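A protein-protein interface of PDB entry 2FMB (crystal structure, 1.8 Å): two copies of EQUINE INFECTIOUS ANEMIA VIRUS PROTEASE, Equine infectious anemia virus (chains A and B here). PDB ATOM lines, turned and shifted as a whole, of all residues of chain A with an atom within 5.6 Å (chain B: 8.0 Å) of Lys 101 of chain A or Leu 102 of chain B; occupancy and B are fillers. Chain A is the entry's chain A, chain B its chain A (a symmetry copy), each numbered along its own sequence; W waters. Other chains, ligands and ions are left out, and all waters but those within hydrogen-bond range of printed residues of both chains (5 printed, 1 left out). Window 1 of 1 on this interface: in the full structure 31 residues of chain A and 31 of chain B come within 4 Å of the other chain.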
ATOM      1  N   VAL A   1      21.823 -11.160 -15.743  1.00  0.00           N
ATOM      2  CA  VAL A   1      21.042 -10.568 -16.873  1.00  0.00           C
ATOM      3  C   VAL A   1      22.011 -10.581 -18.058  1.00  0.00           C
ATOM      4  O   VAL A   1      23.225 -10.604 -17.867  1.00  0.00           O
ATOM      5  CB  VAL A   1      20.225  -9.286 -16.748  1.00  0.00           C
ATOM      6  CG1 VAL A   1      19.770  -8.900 -15.333  1.00  0.00           C
ATOM      7  CG2 VAL A   1      20.926  -8.076 -17.339  1.00  0.00           C
ATOM      8  N   THR A   2      21.426 -10.636 -19.217  1.00  0.00           N
ATOM      9  CA  THR A   2      22.120 -10.753 -20.498  1.00  0.00           C
ATOM     10  C   THR A   2      21.959  -9.475 -21.287  1.00  0.00           C
ATOM     11  O   THR A   2      20.856  -8.952 -21.324  1.00  0.00           O
ATOM     12  CB  THR A   2      21.582 -11.980 -21.259  1.00  0.00           C
ATOM     13  OG1 THR A   2      22.000 -13.162 -20.525  1.00  0.00           O
ATOM     14  CG2 THR A   2      22.220 -12.121 -22.626  1.00  0.00           C
ATOM     15  N   TYR A   3      23.064  -8.944 -21.830  1.00  0.00           N
ATOM     16  CA  TYR A   3      22.929  -7.691 -22.597  1.00  0.00           C
ATOM     17  C   TYR A   3      23.165  -8.121 -24.039  1.00  0.00           C
ATOM     18  O   TYR A   3      24.226  -8.704 -24.314  1.00  0.00           O
ATOM     19  CB  TYR A   3      24.036  -6.696 -22.222  1.00  0.00           C
ATOM     20  CG  TYR A   3      23.840  -6.335 -20.767  1.00  0.00           C
ATOM     21  CD1 TYR A   3      24.336  -7.088 -19.728  1.00  0.00           C
ATOM     22  CD2 TYR A   3      23.153  -5.135 -20.550  1.00  0.00           C
ATOM     23  CE1 TYR A   3      24.095  -6.724 -18.412  1.00  0.00           C
ATOM     24  CE2 TYR A   3      22.970  -4.758 -19.227  1.00  0.00           C
ATOM     25  CZ  TYR A   3      23.405  -5.542 -18.196  1.00  0.00           C
ATOM     26  OH  TYR A   3      23.168  -5.092 -16.912  1.00  0.00           O
ATOM     27  N   ASN A   4      22.217  -7.855 -24.901  1.00  0.00           N
ATOM     28  CA  ASN A   4      22.300  -8.241 -26.307  1.00  0.00           C
ATOM     29  C   ASN A   4      22.946  -7.205 -27.212  1.00  0.00           C
ATOM     30  O   ASN A   4      23.020  -7.338 -28.447  1.00  0.00           O
ATOM     31  CB  ASN A   4      20.894  -8.627 -26.761  1.00  0.00           C
ATOM     32  CG  ASN A   4      19.892  -7.505 -26.924  1.00  0.00           C
ATOM     33  OD1 ASN A   4      20.137  -6.310 -26.745  1.00  0.00           O
ATOM     34  ND2 ASN A   4      18.682  -7.849 -27.371  1.00  0.00           N
ATOM     35  N   LEU A   5      23.350  -6.099 -26.590  1.00  0.00           N
ATOM     36  CA  LEU A   5      24.100  -5.040 -27.258  1.00  0.00           C
ATOM     37  C   LEU A   5      23.383  -4.185 -28.265  1.00  0.00           C
ATOM     38  O   LEU A   5      24.016  -3.393 -28.982  1.00  0.00           O
ATOM     39  CB  LEU A   5      25.436  -5.624 -27.781  1.00  0.00           C
ATOM     40  CG  LEU A   5      26.287  -6.414 -26.775  1.00  0.00           C
ATOM     41  CD1 LEU A   5      27.521  -7.073 -27.392  1.00  0.00           C
ATOM     42  CD2 LEU A   5      26.704  -5.540 -25.601  1.00  0.00           C
ATOM     43  N   PRO A   9      25.414  -1.353 -22.908  1.00  0.00           N
ATOM     44  CA  PRO A   9      25.169  -2.146 -21.717  1.00  0.00           C
ATOM     45  C   PRO A   9      25.472  -1.319 -20.477  1.00  0.00           C
ATOM     46  O   PRO A   9      26.614  -1.147 -20.084  1.00  0.00           O
ATOM     47  CB  PRO A   9      26.093  -3.357 -21.956  1.00  0.00           C
ATOM     48  CG  PRO A   9      27.217  -2.798 -22.747  1.00  0.00           C
ATOM     49  CD  PRO A   9      26.638  -1.752 -23.674  1.00  0.00           C
ATOM     50  N   LEU A  24      29.265  -1.018 -19.062  1.00  0.00           N
ATOM     51  CA  LEU A  24      30.084  -2.251 -18.836  1.00  0.00           C
ATOM     52  C   LEU A  24      30.885  -2.384 -20.154  1.00  0.00           C
ATOM     53  O   LEU A  24      30.335  -2.560 -21.236  1.00  0.00           O
ATOM     54  CB  LEU A  24      29.091  -3.397 -18.727  1.00  0.00           C
ATOM     55  CG  LEU A  24      28.094  -3.118 -17.551  1.00  0.00           C
ATOM     56  CD1 LEU A  24      27.067  -4.259 -17.573  1.00  0.00           C
ATOM     57  CD2 LEU A  24      28.803  -3.140 -16.238  1.00  0.00           C
ATOM     58  N   THR A  26      33.960  -4.094 -22.059  1.00  0.00           N
ATOM     59  CA  THR A  26      35.005  -5.142 -22.195  1.00  0.00           C
ATOM     60  C   THR A  26      36.265  -4.585 -22.856  1.00  0.00           C
ATOM     61  O   THR A  26      37.279  -5.271 -22.733  1.00  0.00           O
ATOM     62  CB  THR A  26      34.531  -6.350 -22.987  1.00  0.00           C
ATOM     63  OG1 THR A  26      34.094  -5.834 -24.255  1.00  0.00           O
ATOM     64  CG2 THR A  26      33.286  -6.955 -22.320  1.00  0.00           C
ATOM     65  N   LEU A  95      34.755  -6.143 -13.826  1.00  0.00           N
ATOM     66  CA  LEU A  95      33.910  -7.084 -14.542  1.00  0.00           C
ATOM     67  C   LEU A  95      34.280  -8.533 -14.175  1.00  0.00           C
ATOM     68  O   LEU A  95      33.448  -9.436 -14.033  1.00  0.00           O
ATOM     69  CB  LEU A  95      33.944  -6.904 -16.059  1.00  0.00           C
ATOM     70  CG  LEU A  95      33.212  -5.636 -16.563  1.00  0.00           C
ATOM     71  CD1 LEU A  95      33.326  -5.535 -18.082  1.00  0.00           C
ATOM     72  CD2 LEU A  95      31.720  -5.669 -16.279  1.00  0.00           C
ATOM     73  N   GLY A  99      32.125 -11.471 -12.111  1.00  0.00           N
ATOM     74  CA  GLY A  99      31.682 -12.671 -12.820  1.00  0.00           C
ATOM     75  C   GLY A  99      31.131 -12.470 -14.195  1.00  0.00           C
ATOM     76  O   GLY A  99      30.485 -13.381 -14.721  1.00  0.00           O
ATOM     77  N   ALA A 100      31.284 -11.309 -14.811  1.00  0.00           N
ATOM     78  CA  ALA A 100      30.739 -11.044 -16.127  1.00  0.00           C
ATOM     79  C   ALA A 100      31.506 -11.831 -17.188  1.00  0.00           C
ATOM     80  O   ALA A 100      32.681 -12.178 -17.081  1.00  0.00           O
ATOM     81  CB  ALA A 100      30.872  -9.567 -16.528  1.00  0.00           C
ATOM     82  N   LYS A 101      30.793 -12.180 -18.219  1.00  0.00           N
ATOM     83  CA  LYS A 101      31.443 -12.920 -19.299  1.00  0.00           C
ATOM     84  C   LYS A 101      30.900 -12.453 -20.647  1.00  0.00           C
ATOM     85  O   LYS A 101      29.735 -12.129 -20.839  1.00  0.00           O
ATOM     86  CB  LYS A 101      31.216 -14.426 -19.115  1.00  0.00           C
ATOM     87  CG  LYS A 101      29.881 -14.828 -19.759  1.00  0.00           C
ATOM     88  CD  LYS A 101      29.639 -16.319 -19.549  1.00  0.00           C
ATOM     89  CE  LYS A 101      29.920 -16.726 -18.102  1.00  0.00           C
ATOM     90  NZ  LYS A 101      28.976 -17.816 -17.685  1.00  0.00           N
ATOM     91  N   LEU A 102      31.803 -12.466 -21.660  1.00  0.00           N
ATOM     92  CA  LEU A 102      31.309 -12.105 -22.975  1.00  0.00           C
ATOM     93  C   LEU A 102      31.264 -13.416 -23.825  1.00  0.00           C
ATOM     94  O   LEU A 102      32.209 -14.195 -23.737  1.00  0.00           O
ATOM     95  CB  LEU A 102      32.470 -11.286 -23.625  1.00  0.00           C
ATOM     96  CG  LEU A 102      32.093 -10.774 -25.002  1.00  0.00           C
ATOM     97  CD1 LEU A 102      30.836  -9.889 -25.051  1.00  0.00           C
ATOM     98  CD2 LEU A 102      33.274  -9.903 -25.496  1.00  0.00           C
ATOM     99  N   VAL A 103      30.151 -13.688 -24.456  1.00  0.00           N
ATOM    100  CA  VAL A 103      30.007 -14.927 -25.201  1.00  0.00           C
ATOM    101  C   VAL A 103      29.847 -14.602 -26.677  1.00  0.00           C
ATOM    102  O   VAL A 103      28.960 -13.839 -27.055  1.00  0.00           O
ATOM    103  CB  VAL A 103      28.687 -15.582 -24.761  1.00  0.00           C
ATOM    104  CG1 VAL A 103      28.539 -16.967 -25.373  1.00  0.00           C
ATOM    105  CG2 VAL A 103      28.621 -15.726 -23.256  1.00  0.00           C
ATOM    106  N   VAL B   1      32.431 -19.272 -27.961  1.00  0.00           N
ATOM    107  CA  VAL B   1      33.525 -19.291 -26.940  1.00  0.00           C
ATOM    108  C   VAL B   1      33.161 -18.166 -25.968  1.00  0.00           C
ATOM    109  O   VAL B   1      32.439 -17.240 -26.331  1.00  0.00           O
ATOM    110  CB  VAL B   1      35.006 -19.354 -27.298  1.00  0.00           C
ATOM    111  CG1 VAL B   1      35.353 -19.937 -28.675  1.00  0.00           C
ATOM    112  CG2 VAL B   1      35.698 -18.007 -27.195  1.00  0.00           C
ATOM    113  N   THR B   2      33.622 -18.340 -24.765  1.00  0.00           N
ATOM    114  CA  THR B   2      33.341 -17.464 -23.628  1.00  0.00           C
ATOM    115  C   THR B   2      34.598 -16.732 -23.223  1.00  0.00           C
ATOM    116  O   THR B   2      35.643 -17.361 -23.165  1.00  0.00           O
ATOM    117  CB  THR B   2      32.755 -18.300 -22.474  1.00  0.00           C
ATOM    118  OG1 THR B   2      31.442 -18.760 -22.894  1.00  0.00           O
ATOM    119  CG2 THR B   2      32.498 -17.459 -21.241  1.00  0.00           C
ATOM    120  N   TYR B   3      34.504 -15.407 -23.034  1.00  0.00           N
ATOM    121  CA  TYR B   3      35.722 -14.672 -22.647  1.00  0.00           C
ATOM    122  C   TYR B   3      35.465 -14.282 -21.196  1.00  0.00           C
ATOM    123  O   TYR B   3      34.443 -13.627 -20.935  1.00  0.00           O
ATOM    124  CB  TYR B   3      35.863 -13.377 -23.458  1.00  0.00           C
ATOM    125  CG  TYR B   3      36.040 -13.773 -24.907  1.00  0.00           C
ATOM    126  CD1 TYR B   3      34.988 -14.042 -25.751  1.00  0.00           C
ATOM    127  CD2 TYR B   3      37.368 -13.797 -25.347  1.00  0.00           C
ATOM    128  CE1 TYR B   3      35.213 -14.433 -27.062  1.00  0.00           C
ATOM    129  CE2 TYR B   3      37.572 -14.137 -26.678  1.00  0.00           C
ATOM    130  CZ  TYR B   3      36.529 -14.467 -27.497  1.00  0.00           C
ATOM    131  OH  TYR B   3      36.827 -14.804 -28.801  1.00  0.00           O
ATOM    132  N   ASN B   4      36.342 -14.677 -20.309  1.00  0.00           N
ATOM    133  CA  ASN B   4      36.200 -14.399 -18.883  1.00  0.00           C
ATOM    134  C   ASN B   4      36.830 -13.095 -18.425  1.00  0.00           C
ATOM    135  O   ASN B   4      36.873 -12.747 -17.230  1.00  0.00           O
ATOM    136  CB  ASN B   4      36.735 -15.612 -18.125  1.00  0.00           C
ATOM    137  CG  ASN B   4      38.233 -15.824 -18.135  1.00  0.00           C
ATOM    138  OD1 ASN B   4      39.046 -15.077 -18.684  1.00  0.00           O
ATOM    139  ND2 ASN B   4      38.692 -16.857 -17.425  1.00  0.00           N
ATOM    140  N   LEU B   5      37.413 -12.389 -19.393  1.00  0.00           N
ATOM    141  CA  LEU B   5      37.967 -11.056 -19.181  1.00  0.00           C
ATOM    142  C   LEU B   5      39.221 -10.926 -18.362  1.00  0.00           C
ATOM    143  O   LEU B   5      39.628  -9.807 -18.009  1.00  0.00           O
ATOM    144  CB  LEU B   5      36.830 -10.106 -18.727  1.00  0.00           C
ATOM    145  CG  LEU B   5      35.556 -10.093 -19.586  1.00  0.00           C
ATOM    146  CD1 LEU B   5      34.428  -9.238 -19.006  1.00  0.00           C
ATOM    147  CD2 LEU B   5      35.855  -9.652 -21.010  1.00  0.00           C
ATOM    148  N   THR B  26      32.461  -4.011 -25.904  1.00  0.00           N
ATOM    149  CA  THR B  26      31.047  -3.642 -25.639  1.00  0.00           C
ATOM    150  C   THR B  26      30.906  -2.144 -25.370  1.00  0.00           C
ATOM    151  O   THR B  26      29.764  -1.694 -25.448  1.00  0.00           O
ATOM    152  CB  THR B  26      30.445  -4.406 -24.470  1.00  0.00           C
ATOM    153  OG1 THR B  26      31.307  -4.143 -23.351  1.00  0.00           O
ATOM    154  CG2 THR B  26      30.537  -5.918 -24.733  1.00  0.00           C
ATOM    155  N   GLY B  27      31.947  -1.422 -25.026  1.00  0.00           N
ATOM    156  CA  GLY B  27      31.962   0.027 -24.809  1.00  0.00           C
ATOM    157  C   GLY B  27      32.091   0.769 -26.114  1.00  0.00           C
ATOM    158  O   GLY B  27      32.272   1.990 -26.005  1.00  0.00           O
ATOM    159  N   LEU B  95      29.062  -6.741 -33.225  1.00  0.00           N
ATOM    160  CA  LEU B  95      28.873  -7.698 -32.147  1.00  0.00           C
ATOM    161  C   LEU B  95      27.426  -8.225 -32.138  1.00  0.00           C
ATOM    162  O   LEU B  95      27.128  -9.397 -31.883  1.00  0.00           O
ATOM    163  CB  LEU B  95      29.238  -7.145 -30.770  1.00  0.00           C
ATOM    164  CG  LEU B  95      30.759  -6.965 -30.542  1.00  0.00           C
ATOM    165  CD1 LEU B  95      31.015  -6.387 -29.153  1.00  0.00           C
ATOM    166  CD2 LEU B  95      31.515  -8.283 -30.569  1.00  0.00           C
ATOM    167  N   GLY B  99      25.898 -12.045 -32.912  1.00  0.00           N
ATOM    168  CA  GLY B  99      25.273 -12.804 -31.830  1.00  0.00           C
ATOM    169  C   GLY B  99      25.958 -12.761 -30.502  1.00  0.00           C
ATOM    170  O   GLY B  99      25.653 -13.594 -29.642  1.00  0.00           O
ATOM    171  N   ALA B 100      26.918 -11.879 -30.275  1.00  0.00           N
ATOM    172  CA  ALA B 100      27.641 -11.816 -29.022  1.00  0.00           C
ATOM    173  C   ALA B 100      26.738 -11.278 -27.912  1.00  0.00           C
ATOM    174  O   ALA B 100      25.786 -10.522 -28.098  1.00  0.00           O
ATOM    175  CB  ALA B 100      28.837 -10.854 -29.085  1.00  0.00           C
ATOM    176  N   LYS B 101      27.009 -11.741 -26.727  1.00  0.00           N
ATOM    177  CA  LYS B 101      26.213 -11.270 -25.595  1.00  0.00           C
ATOM    178  C   LYS B 101      27.105 -11.095 -24.371  1.00  0.00           C
ATOM    179  O   LYS B 101      28.046 -11.831 -24.099  1.00  0.00           O
ATOM    180  CB  LYS B 101      25.079 -12.262 -25.304  1.00  0.00           C
ATOM    181  CG  LYS B 101      25.590 -13.370 -24.371  1.00  0.00           C
ATOM    182  CD  LYS B 101      24.473 -14.373 -24.105  1.00  0.00           C
ATOM    183  CE  LYS B 101      23.759 -14.761 -25.401  1.00  0.00           C
ATOM    184  NZ  LYS B 101      23.327 -16.197 -25.336  1.00  0.00           N
ATOM    185  N   LEU B 102      26.752 -10.073 -23.549  1.00  0.00           N
ATOM    186  CA  LEU B 102      27.526  -9.921 -22.332  1.00  0.00           C
ATOM    187  C   LEU B 102      26.612 -10.370 -21.147  1.00  0.00           C
ATOM    188  O   LEU B 102      25.437 -10.012 -21.154  1.00  0.00           O
ATOM    189  CB  LEU B 102      27.653  -8.376 -22.134  1.00  0.00           C
ATOM    190  CG  LEU B 102      28.496  -8.035 -20.919  1.00  0.00           C
ATOM    191  CD1 LEU B 102      29.923  -8.606 -20.930  1.00  0.00           C
ATOM    192  CD2 LEU B 102      28.629  -6.493 -20.885  1.00  0.00           C
ATOM    193  N   VAL B 103      27.106 -11.235 -20.299  1.00  0.00           N
ATOM    194  CA  VAL B 103      26.288 -11.759 -19.217  1.00  0.00           C
ATOM    195  C   VAL B 103      26.874 -11.305 -17.890  1.00  0.00           C
ATOM    196  O   VAL B 103      28.047 -11.541 -17.612  1.00  0.00           O
ATOM    197  CB  VAL B 103      26.417 -13.292 -19.241  1.00  0.00           C
ATOM    198  CG1 VAL B 103      25.462 -13.930 -18.243  1.00  0.00           C
ATOM    199  CG2 VAL B 103      26.101 -13.849 -20.611  1.00  0.00           C
ATOM    200  N   LEU B 104      26.014 -10.723 -17.068  1.00  0.00           N
ATOM    201  CA  LEU B 104      26.448 -10.276 -15.734  1.00  0.00           C
ATOM    202  C   LEU B 104      25.548 -11.039 -14.755  1.00  0.00           C
ATOM    203  O   LEU B 104      25.962 -11.974 -14.046  1.00  0.00           O
ATOM    204  CB  LEU B 104      26.216  -8.784 -15.570  1.00  0.00           C
ATOM    205  CG  LEU B 104      27.119  -7.957 -14.646  1.00  0.00           C
ATOM    206  CD1 LEU B 104      26.254  -6.922 -13.936  1.00  0.00           C
ATOM    207  CD2 LEU B 104      27.941  -8.707 -13.610  1.00  0.00           C
ATOM    208  OXT LEU B 104      24.362 -10.660 -14.821  1.00  0.00           O
HETATM  209  O   HOH W   1      22.527 -15.770 -22.114  1.00  0.00           O
HETATM  210  O   HOH W   2      26.774 -15.644 -28.121  1.00  0.00           O
HETATM  211  O   HOH W   3      34.631 -13.236 -15.489  1.00  0.00           O
HETATM  212  O   HOH W   4      29.266 -19.178 -20.728  1.00  0.00           O
HETATM  213  O   HOH W   5      23.592  -9.913 -29.604  1.00  0.00           O
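N of Val 103 of chain A is in hydrogen-bond range of O of Lys 101 of chain B (2.8 Å).
O of Leu 102 of chain A sits at hydrogen-bond distance from N of Tyr 3 of chain B (2.7 Å).
The backbone NH of Val 1 of chain A sits at hydrogen-bond distance from the chain-end carboxylate of Leu 104 of chain B, 2.7 Å away.
N of Tyr 3 of chain A lies within hydrogen-bond range of O of Leu 102 of chain B, 2.7 Å away.
O of Lys 101 of chain A sits at hydrogen-bond distance from N of Val 103 of chain B, 2.8 Å away.
The backbone NH (N) of Thr 26 of chain A is in hydrogen-bond range of the side-chain hydroxyl (OG1) of Thr 26 of chain B (3.0 Å).
O of Leu 24 of chain A is in hydrogen-bond range of OG1 of Thr 26 of chain B.
The backbone carbonyl oxygen (O) of Leu 95 of chain A lies within hydrogen-bond range of the backbone NH (N) of Ala 100 of chain A, at 3.0 Å.
O of Pro 9 of chain A sits at hydrogen-bond distance from N of Leu 24 of chain A (2.8 Å).
N of Ala 100 of chain B lies within hydrogen-bond range of O of Leu 95 of chain B, at 3.0 Å.
Lys 101 of chain A touches just these residues of chain B: Thr 2 (3.5 Å), Tyr 3 (3.5 Å), Lys 101 (3.7 Å), Leu 102 (3.5 Å) and Val 103 (2.8 Å).
Printed residues of chain A within 4 Å of Leu 102 of chain B: Thr 2, Tyr 3, Leu 24, Thr 26 and Lys 101.
Ala 100 of chain A touches just these residues of chain B: Leu 5 and Val 103.
Printed residues of chain B within 4 Å of Leu 5 of chain A: Thr 26, Leu 95 and Ala 100.
Of the printed residues of chain B, Tyr 3 of chain A touches Lys 101 (3.5 Å) and Leu 102 (2.7 Å).
Printed residues of chain B within 4 Å of Thr 26 of chain A: Leu 5, Thr 26 and Leu 102.
Of the printed residues of chain A, Lys 101 of chain B touches Thr 2 (3.5 Å), Tyr 3 (3.5 Å), Lys 101 (3.7 Å), Leu 102 (3.5 Å) and Val 103 (2.8 Å).
Gly 99 of chain A touches none of the printed residues of chain B.
Gly 99 of chain B touches none of the printed residues of chain A.
The nearest residue of chain B that does not touch Lys 101 of chain A is Leu 5 of chain B (4.7 Å).
The nearest printed residue of chain A that does not touch Leu 102 of chain B is Val 1 of chain A (4.01 Å).
Of the 14 printed residues of chain A, 12 touch a printed residue of chain B.
Printed residues of chain A that touch a printed residue of chain B: Val 1, Thr 2, Tyr 3, Leu 5, Pro 9, Leu 24, Thr 26, Leu 95, Ala 100, Lys 101, Leu 102 and Val 103.
Hydrophobic or aromatic side chains of chain A that line the printed part of chain B: Tyr 3, Leu 5, Pro 9, Leu 24, Leu 95, Ala 100, Leu 102 and Val 103.
Of the 14 printed residues of chain B, 11 touch a printed residue of chain A.
Hydrophobic or aromatic side chains of chain B within 4 Å of the printed part of chain A: Tyr 3, Leu 5, Leu 95, Ala 100, Leu 102 and Val 103.
Among the printed residues, 30 pairs touch across the chains.
Among the printed residues, no Asp or Glu carboxylate lies within 4 Å of a Lys or Arg side-chain nitrogen of the other chain.
Water W3 bridges the backbone carbonyl oxygen (O) of Ala 100 of chain A (2.7 Å) and the backbone carbonyl oxygen (O) of Asn 4 of chain B (2.9 Å).
Water W5 bridges the backbone carbonyl oxygen (O) of Ala 100 of chain B (2.7 Å) and the backbone carbonyl oxygen (O) of Asn 4 of chain A (2.9 Å).
Water W2 bridges the backbone carbonyl oxygen (O) of Gly 99 of chain B and the backbone carbonyl oxygen (O) of Val 103 of chain A.
Water W1 lies within hydrogen-bond range of the side-chain hydroxyl (OG1) of Thr 2 of chain A and the side-chain amino group (NZ) of Lys 101 of chain B.
Water W4 bridges OG1 of Thr 2 of chain B and NZ of Lys 101 of chain A.
Val 1 of chain A touches Val 103 of chain B, and with the chains exchanged Val 103 of chain A touches Val 1 of chain B.
Tyr 3 of chain A touches Leu 102 of chain B, and with the chains exchanged Leu 102 of chain A touches Tyr 3 of chain B.
Leu 5 of chain A touches Ala 100 of chain B, and with the chains exchanged Ala 100 of chain A touches Leu 5 of chain B.
Lys 101 of chain A touches Leu 102 of chain B, and with the chains exchanged Leu 102 of chain A touches Lys 101 of chain B.
Of the 30 pairs that touch across the chains among the printed residues, 26 have their exchanged pair printed and touching as well.
Among the printed residues, merely in contact across the chains: Val 1 of chain A with Val 103 of chain B, Thr 2 of chain A with Lys 101 of chain B, Thr 2 of chain A with Leu 102 of chain B, Tyr 3 of chain A with Lys 101 of chain B, Leu 5 of chain A with Thr 26 of chain B, Leu 5 of chain A with Leu 95 of chain B, Leu 5 of chain A with Ala 100 of chain B, Pro 9 of chain A with Thr 26 of chain B, Leu 24 of chain A with Leu 102 of chain B, Thr 26 of chain A with Leu 5 of chain B, Thr 26 of chain A with Leu 102 of chain B, Leu 95 of chain A with Leu 5 of chain B, Ala 100 of chain A with Leu 5 of chain B, Ala 100 of chain A with Val 103 of chain B, Lys 101 of chain A with Thr 2 of chain B, Lys 101 of chain A with Tyr 3 of chain B, Lys 101 of chain A with Lys 101 of chain B, Lys 101 of chain A with Leu 102 of chain B, Leu 102 of chain A with Thr 2 of chain B, Leu 102 of chain A with Thr 26 of chain B, Leu 102 of chain A with Lys 101 of chain B, Val 103 of chain A with Val 1 of chain B and Val 103 of chain A with Ala 100 of chain B.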
